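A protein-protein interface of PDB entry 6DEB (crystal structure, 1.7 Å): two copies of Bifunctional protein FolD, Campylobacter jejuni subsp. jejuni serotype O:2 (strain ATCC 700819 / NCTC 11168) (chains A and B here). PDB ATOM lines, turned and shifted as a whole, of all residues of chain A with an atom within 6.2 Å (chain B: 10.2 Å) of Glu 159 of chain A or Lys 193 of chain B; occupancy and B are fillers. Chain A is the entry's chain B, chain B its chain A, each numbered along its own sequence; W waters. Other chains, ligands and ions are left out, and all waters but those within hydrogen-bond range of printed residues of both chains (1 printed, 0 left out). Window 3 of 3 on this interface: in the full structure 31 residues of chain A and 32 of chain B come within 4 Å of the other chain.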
ATOM      1  N   ASP A 157      -8.990  28.486 -16.443  1.00  0.00           N
ATOM      2  CA  ASP A 157      -8.258  27.294 -16.877  1.00  0.00           C
ATOM      3  C   ASP A 157      -6.771  27.607 -16.963  1.00  0.00           C
ATOM      4  O   ASP A 157      -6.362  28.550 -17.632  1.00  0.00           O
ATOM      5  CB  ASP A 157      -8.775  26.800 -18.239  1.00  0.00           C
ATOM      6  CG  ASP A 157      -7.904  25.689 -18.836  1.00  0.00           C
ATOM      7  OD1 ASP A 157      -7.519  24.749 -18.100  1.00  0.00           O
ATOM      8  OD2 ASP A 157      -7.594  25.761 -20.049  1.00  0.00           O
ATOM      9  N   LEU A 158      -5.957  26.824 -16.265  1.00  0.00           N
ATOM     10  CA  LEU A 158      -4.537  27.131 -16.160  1.00  0.00           C
ATOM     11  C   LEU A 158      -3.692  26.343 -17.162  1.00  0.00           C
ATOM     12  O   LEU A 158      -2.550  26.694 -17.426  1.00  0.00           O
ATOM     13  CB  LEU A 158      -4.054  26.832 -14.744  1.00  0.00           C
ATOM     14  CG  LEU A 158      -4.810  27.651 -13.694  1.00  0.00           C
ATOM     15  CD1 LEU A 158      -4.398  27.204 -12.306  1.00  0.00           C
ATOM     16  CD2 LEU A 158      -4.488  29.145 -13.857  1.00  0.00           C
ATOM     17  N   GLU A 159      -4.254  25.291 -17.740  1.00  0.00           N
ATOM     18  CA  GLU A 159      -3.443  24.413 -18.579  1.00  0.00           C
ATOM     19  C   GLU A 159      -2.939  25.170 -19.801  1.00  0.00           C
ATOM     20  O   GLU A 159      -3.724  25.825 -20.489  1.00  0.00           O
ATOM     21  CB  GLU A 159      -4.257  23.194 -19.013  1.00  0.00           C
ATOM     22  CG  GLU A 159      -3.424  22.130 -19.697  1.00  0.00           C
ATOM     23  CD  GLU A 159      -4.226  20.878 -20.029  1.00  0.00           C
ATOM     24  OE1 GLU A 159      -4.084  20.373 -21.157  1.00  0.00           O
ATOM     25  OE2 GLU A 159      -4.996  20.403 -19.166  1.00  0.00           O
ATOM     26  N   GLY A 160      -1.630  25.095 -20.053  1.00  0.00           N
ATOM     27  CA  GLY A 160      -1.045  25.758 -21.208  1.00  0.00           C
ATOM     28  C   GLY A 160      -0.832  27.260 -21.036  1.00  0.00           C
ATOM     29  O   GLY A 160      -0.264  27.898 -21.912  1.00  0.00           O
ATOM     30  N   LYS A 161      -1.268  27.838 -19.921  1.00  0.00           N
ATOM     31  CA  LYS A 161      -1.104  29.278 -19.738  1.00  0.00           C
ATOM     32  C   LYS A 161       0.348  29.653 -19.491  1.00  0.00           C
ATOM     33  O   LYS A 161       1.093  28.882 -18.898  1.00  0.00           O
ATOM     34  CB  LYS A 161      -1.961  29.792 -18.571  1.00  0.00           C
ATOM     35  CG  LYS A 161      -3.469  29.787 -18.850  1.00  0.00           C
ATOM     36  CD  LYS A 161      -3.809  30.308 -20.240  1.00  0.00           C
ATOM     37  CE  LYS A 161      -5.270  30.014 -20.616  1.00  0.00           C
ATOM     38  NZ  LYS A 161      -5.627  30.611 -21.942  1.00  0.00           N
ATOM     39  N   ALA A 183      -0.435  22.282 -12.360  1.00  0.00           N
ATOM     40  CA  ALA A 183      -1.708  22.533 -13.032  1.00  0.00           C
ATOM     41  C   ALA A 183      -1.555  22.658 -14.543  1.00  0.00           C
ATOM     42  O   ALA A 183      -2.553  22.823 -15.270  1.00  0.00           O
ATOM     43  CB  ALA A 183      -2.358  23.790 -12.454  1.00  0.00           C
ATOM     44  N   GLY A 184      -0.315  22.568 -15.012  1.00  0.00           N
ATOM     45  CA  GLY A 184      -0.050  22.444 -16.434  1.00  0.00           C
ATOM     46  C   GLY A 184       0.287  23.774 -17.083  1.00  0.00           C
ATOM     47  O   GLY A 184       0.385  23.856 -18.310  1.00  0.00           O
ATOM     48  N   ALA A 185       0.456  24.809 -16.271  1.00  0.00           N
ATOM     49  CA  ALA A 185       0.937  26.088 -16.803  1.00  0.00           C
ATOM     50  C   ALA A 185       2.425  26.033 -17.130  1.00  0.00           C
ATOM     51  O   ALA A 185       3.174  25.240 -16.565  1.00  0.00           O
ATOM     52  CB  ALA A 185       0.654  27.221 -15.826  1.00  0.00           C
ATOM     53  N   THR A 186       2.854  26.865 -18.060  1.00  0.00           N
ATOM     54  CA  THR A 186       4.291  27.123 -18.247  1.00  0.00           C
ATOM     55  C   THR A 186       4.652  28.222 -17.257  1.00  0.00           C
ATOM     56  O   THR A 186       3.946  29.237 -17.178  1.00  0.00           O
ATOM     57  CB  THR A 186       4.562  27.597 -19.678  1.00  0.00           C
ATOM     58  OG1 THR A 186       4.138  26.588 -20.598  1.00  0.00           O
ATOM     59  CG2 THR A 186       6.061  27.859 -19.847  1.00  0.00           C
ATOM     60  N   ILE B 166      13.612  22.703 -20.415  1.00  0.00           N
ATOM     61  CA  ILE B 166      12.589  22.024 -21.193  1.00  0.00           C
ATOM     62  C   ILE B 166      12.400  20.627 -20.639  1.00  0.00           C
ATOM     63  O   ILE B 166      13.293  19.776 -20.743  1.00  0.00           O
ATOM     64  CB  ILE B 166      12.997  21.970 -22.681  1.00  0.00           C
ATOM     65  CG1 ILE B 166      13.425  23.387 -23.126  1.00  0.00           C
ATOM     66  CG2 ILE B 166      11.867  21.356 -23.514  1.00  0.00           C
ATOM     67  CD1 ILE B 166      13.947  23.476 -24.557  1.00  0.00           C
ATOM     68  N   GLY B 167      11.261  20.410 -19.992  1.00  0.00           N
ATOM     69  CA  GLY B 167      10.988  19.139 -19.334  1.00  0.00           C
ATOM     70  C   GLY B 167      10.802  19.405 -17.848  1.00  0.00           C
ATOM     71  O   GLY B 167      11.609  20.114 -17.256  1.00  0.00           O
ATOM     72  N   ALA B 168       9.748  18.850 -17.271  1.00  0.00           N
ATOM     73  CA  ALA B 168       9.445  19.116 -15.862  1.00  0.00           C
ATOM     74  C   ALA B 168       9.395  17.836 -15.035  1.00  0.00           C
ATOM     75  O   ALA B 168       8.545  17.697 -14.152  1.00  0.00           O
ATOM     76  CB  ALA B 168       8.125  19.888 -15.743  1.00  0.00           C
ATOM     77  N   ARG B 174      12.557  19.524 -12.777  1.00  0.00           N
ATOM     78  CA  ARG B 174      12.181  20.288 -11.578  1.00  0.00           C
ATOM     79  C   ARG B 174      13.392  20.596 -10.679  1.00  0.00           C
ATOM     80  O   ARG B 174      13.624  21.762 -10.354  1.00  0.00           O
ATOM     81  CB  ARG B 174      11.073  19.574 -10.821  1.00  0.00           C
ATOM     82  CG  ARG B 174       9.748  19.661 -11.586  1.00  0.00           C
ATOM     83  CD  ARG B 174       8.723  18.744 -10.995  1.00  0.00           C
ATOM     84  NE  ARG B 174       7.459  18.798 -11.745  1.00  0.00           N
ATOM     85  CZ  ARG B 174       6.294  19.189 -11.234  1.00  0.00           C
ATOM     86  NH1 ARG B 174       6.205  19.544  -9.952  1.00  0.00           N
ATOM     87  NH2 ARG B 174       5.198  19.194 -11.995  1.00  0.00           N
ATOM     88  N   VAL B 189      10.134  27.059 -16.847  1.00  0.00           N
ATOM     89  CA  VAL B 189      10.022  25.626 -17.034  1.00  0.00           C
ATOM     90  C   VAL B 189       8.962  25.360 -18.083  1.00  0.00           C
ATOM     91  O   VAL B 189       7.775  25.698 -17.909  1.00  0.00           O
ATOM     92  CB  VAL B 189       9.658  24.907 -15.725  1.00  0.00           C
ATOM     93  CG1 VAL B 189       9.541  23.413 -15.955  1.00  0.00           C
ATOM     94  CG2 VAL B 189      10.740  25.197 -14.656  1.00  0.00           C
ATOM     95  N   CYS B 190       9.399  24.766 -19.193  1.00  0.00           N
ATOM     96  CA  CYS B 190       8.527  24.456 -20.319  1.00  0.00           C
ATOM     97  C   CYS B 190       8.317  22.955 -20.396  1.00  0.00           C
ATOM     98  O   CYS B 190       9.107  22.192 -19.849  1.00  0.00           O
ATOM     99  CB  CYS B 190       9.166  24.943 -21.615  1.00  0.00           C
ATOM    100  SG  CYS B 190       9.448  26.725 -21.632  1.00  0.00           S
ATOM    101  N   HIS B 191       7.249  22.543 -21.080  1.00  0.00           N
ATOM    102  CA  HIS B 191       6.869  21.137 -21.099  1.00  0.00           C
ATOM    103  C   HIS B 191       5.895  20.920 -22.246  1.00  0.00           C
ATOM    104  O   HIS B 191       5.750  21.793 -23.096  1.00  0.00           O
ATOM    105  CB  HIS B 191       6.285  20.691 -19.742  1.00  0.00           C
ATOM    106  CG  HIS B 191       5.301  21.659 -19.165  1.00  0.00           C
ATOM    107  ND1 HIS B 191       4.012  21.772 -19.629  1.00  0.00           N
ATOM    108  CD2 HIS B 191       5.434  22.598 -18.192  1.00  0.00           C
ATOM    109  CE1 HIS B 191       3.377  22.710 -18.944  1.00  0.00           C
ATOM    110  NE2 HIS B 191       4.223  23.234 -18.070  1.00  0.00           N
ATOM    111  N   ILE B 192       5.230  19.767 -22.271  1.00  0.00           N
ATOM    112  CA  ILE B 192       4.403  19.367 -23.398  1.00  0.00           C
ATOM    113  C   ILE B 192       3.168  20.272 -23.574  1.00  0.00           C
ATOM    114  O   ILE B 192       2.554  20.293 -24.637  1.00  0.00           O
ATOM    115  CB  ILE B 192       3.975  17.877 -23.254  1.00  0.00           C
ATOM    116  CG1 ILE B 192       3.394  17.336 -24.567  1.00  0.00           C
ATOM    117  CG2 ILE B 192       3.004  17.696 -22.101  1.00  0.00           C
ATOM    118  CD1 ILE B 192       4.396  17.319 -25.691  1.00  0.00           C
ATOM    119  N   LYS B 193       2.798  21.010 -22.528  1.00  0.00           N
ATOM    120  CA  LYS B 193       1.613  21.858 -22.605  1.00  0.00           C
ATOM    121  C   LYS B 193       1.941  23.315 -22.928  1.00  0.00           C
ATOM    122  O   LYS B 193       1.026  24.133 -23.097  1.00  0.00           O
ATOM    123  CB  LYS B 193       0.778  21.744 -21.327  1.00  0.00           C
ATOM    124  CG  LYS B 193       0.303  20.336 -21.067  1.00  0.00           C
ATOM    125  CD  LYS B 193      -0.474  20.236 -19.776  1.00  0.00           C
ATOM    126  CE  LYS B 193      -1.064  18.843 -19.622  1.00  0.00           C
ATOM    127  NZ  LYS B 193      -1.701  18.412 -20.893  1.00  0.00           N
ATOM    128  N   THR B 194       3.233  23.617 -23.033  1.00  0.00           N
ATOM    129  CA  THR B 194       3.700  24.953 -23.392  1.00  0.00           C
ATOM    130  C   THR B 194       3.238  25.293 -24.807  1.00  0.00           C
ATOM    131  O   THR B 194       3.471  24.530 -25.741  1.00  0.00           O
ATOM    132  CB  THR B 194       5.223  25.045 -23.307  1.00  0.00           C
ATOM    133  OG1 THR B 194       5.632  24.756 -21.959  1.00  0.00           O
ATOM    134  CG2 THR B 194       5.712  26.444 -23.713  1.00  0.00           C
ATOM    135  N   LYS B 195       2.593  26.441 -24.951  1.00  0.00           N
ATOM    136  CA  LYS B 195       2.037  26.854 -26.238  1.00  0.00           C
ATOM    137  C   LYS B 195       3.081  27.146 -27.305  1.00  0.00           C
ATOM    138  O   LYS B 195       2.924  26.748 -28.469  1.00  0.00           O
ATOM    139  CB  LYS B 195       1.125  28.076 -26.060  1.00  0.00           C
ATOM    140  CG  LYS B 195      -0.149  27.764 -25.264  1.00  0.00           C
ATOM    141  CD  LYS B 195      -1.083  28.970 -25.176  1.00  0.00           C
ATOM    142  CE  LYS B 195      -0.495  30.057 -24.272  1.00  0.00           C
ATOM    143  NZ  LYS B 195      -1.454  31.180 -24.052  1.00  0.00           N
ATOM    144  N   ASP B 196       4.128  27.864 -26.923  1.00  0.00           N
ATOM    145  CA  ASP B 196       5.142  28.272 -27.888  1.00  0.00           C
ATOM    146  C   ASP B 196       6.514  28.206 -27.263  1.00  0.00           C
ATOM    147  O   ASP B 196       7.002  29.190 -26.720  1.00  0.00           O
ATOM    148  CB  ASP B 196       4.854  29.689 -28.399  1.00  0.00           C
ATOM    149  CG  ASP B 196       5.802  30.119 -29.502  1.00  0.00           C
ATOM    150  OD1 ASP B 196       6.642  29.297 -29.949  1.00  0.00           O
ATOM    151  OD2 ASP B 196       5.687  31.285 -29.933  1.00  0.00           O
ATOM    152  N   LEU B 197       7.137  27.040 -27.355  1.00  0.00           N
ATOM    153  CA  LEU B 197       8.454  26.832 -26.767  1.00  0.00           C
ATOM    154  C   LEU B 197       9.504  27.838 -27.271  1.00  0.00           C
ATOM    155  O   LEU B 197      10.334  28.330 -26.506  1.00  0.00           O
ATOM    156  CB  LEU B 197       8.903  25.408 -27.054  1.00  0.00           C
ATOM    157  CG  LEU B 197      10.317  25.015 -26.701  1.00  0.00           C
ATOM    158  CD1 LEU B 197      10.557  25.231 -25.193  1.00  0.00           C
ATOM    159  CD2 LEU B 197      10.548  23.558 -27.107  1.00  0.00           C
ATOM    160  N   TYR B 200      10.198  31.159 -25.573  1.00  0.00           N
ATOM    161  CA  TYR B 200      11.062  31.106 -24.409  1.00  0.00           C
ATOM    162  C   TYR B 200      12.531  30.873 -24.791  1.00  0.00           C
ATOM    163  O   TYR B 200      13.442  31.498 -24.244  1.00  0.00           O
ATOM    164  CB  TYR B 200      10.604  29.994 -23.465  1.00  0.00           C
ATOM    165  CG  TYR B 200       9.320  30.305 -22.750  1.00  0.00           C
ATOM    166  CD1 TYR B 200       9.333  30.931 -21.505  1.00  0.00           C
ATOM    167  CD2 TYR B 200       8.089  29.959 -23.304  1.00  0.00           C
ATOM    168  CE1 TYR B 200       8.161  31.225 -20.849  1.00  0.00           C
ATOM    169  CE2 TYR B 200       6.888  30.245 -22.638  1.00  0.00           C
ATOM    170  CZ  TYR B 200       6.952  30.876 -21.399  1.00  0.00           C
ATOM    171  OH  TYR B 200       5.795  31.171 -20.726  1.00  0.00           O
HETATM  172  O   HOH W   1       2.450  27.933 -22.412  1.00  0.00           O
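O of Lys 193 of chain B touches CA of Gly 160 of chain A, 3.2 Å away.
Gly 160 of chain A touches Lys 195 of chain B (O to CE, 3.2 Å).
Gly 184 of chain A touches His 191 of chain B.
Lys 193 of chain B touches Gly 184 of chain A.
O of Val 189 of chain B touches CG2 of Thr 186 of chain A (3.4 Å).
Cys 190 of chain B touches Thr 186 of chain A (SG to CG2, 3.99 Å).
N of Thr 186 of chain A touches NE2 of His 191 of chain B, at 3.9 Å.
Tyr 200 of chain B touches Thr 186 of chain A (OH to CG2, 3.4 Å).
O of Cys 190 of chain B sits at hydrogen-bond distance from N of Gly 167 of chain B, 2.8 Å away.
N of Lys 193 of chain B lies close to ND1 of His 191 of chain B (3.2 Å).
N of His 191 of chain B sits at hydrogen-bond distance from OG1 of Thr 194 of chain B.
OD1 of Asp 157 of chain A is in hydrogen-bond range of N of Glu 159 of chain A, 3.3 Å away.
N of Gly 160 of chain A lies within hydrogen-bond range of O of Gly 184 of chain A (2.9 Å).
The backbone NH of Thr 186 of chain A sits at hydrogen-bond distance from the backbone carbonyl oxygen of Lys 161 of chain A (2.8 Å).
No position is printed for both chains.
Of the 11 pairs that touch across the chains among the printed residues, none has its exchanged pair printed and touching as well.
NE2 of His 191 of chain B is in hydrogen-bond range of O of Ala 185 of chain A.
The side-chain amino group of Lys 193 of chain B is in salt-bridge range of the side-chain carboxylate of Glu 159 of chain A (3.1 Å).
OG1 of Thr 194 of chain B lies within hydrogen-bond range of OG1 of Thr 186 of chain A (2.7 Å).
Water W1 lies within hydrogen-bond range of the backbone carbonyl oxygen of Gly 160 of chain A (2.8 Å), the side-chain hydroxyl of Thr 186 of chain A (2.8 Å) and the backbone NH of Lys 195 of chain B (2.9 Å).
No residue of chain B comes within 4 Å of Asp 157 of chain A.
No residue of chain B comes within 4 Å of Leu 158 of chain A.
Of chain B, only Lys 193 comes within 4 Å of Glu 159 of chain A.
Of chain B, only Lys 193 (3.2 Å) and Lys 195 (3.2 Å) come within 4 Å of Gly 160 of chain A.
No residue of chain B comes within 4 Å of Lys 161 of chain A.
Gly 184 of chain A touches just these residues of chain B: His 191 and Lys 193.
Of the printed residues of chain B, Ala 185 of chain A touches His 191.
Of the printed residues of chain A, Val 189 of chain B touches Thr 186.
Of the printed residues of chain A, His 191 of chain B touches Gly 184, Ala 185 and Thr 186.
Lys 193 of chain B touches just these residues of chain A: Glu 159 (3.1 Å), Gly 160 (3.2 Å) and Gly 184 (3.7 Å).
Of the printed residues of chain A, Lys 195 of chain B touches Gly 160.
The nearest residue of chain A that does not touch Lys 193 of chain B is Thr 186 of chain A (4.6 Å).
Printed residues of chain B that touch a printed residue of chain A: Val 189, Cys 190, His 191, Lys 193, Thr 194, Lys 195 and Tyr 200.
Of the 9 printed residues of chain A, 5 touch a printed residue of chain B.
Among the printed residues, 11 pairs touch across the chains.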
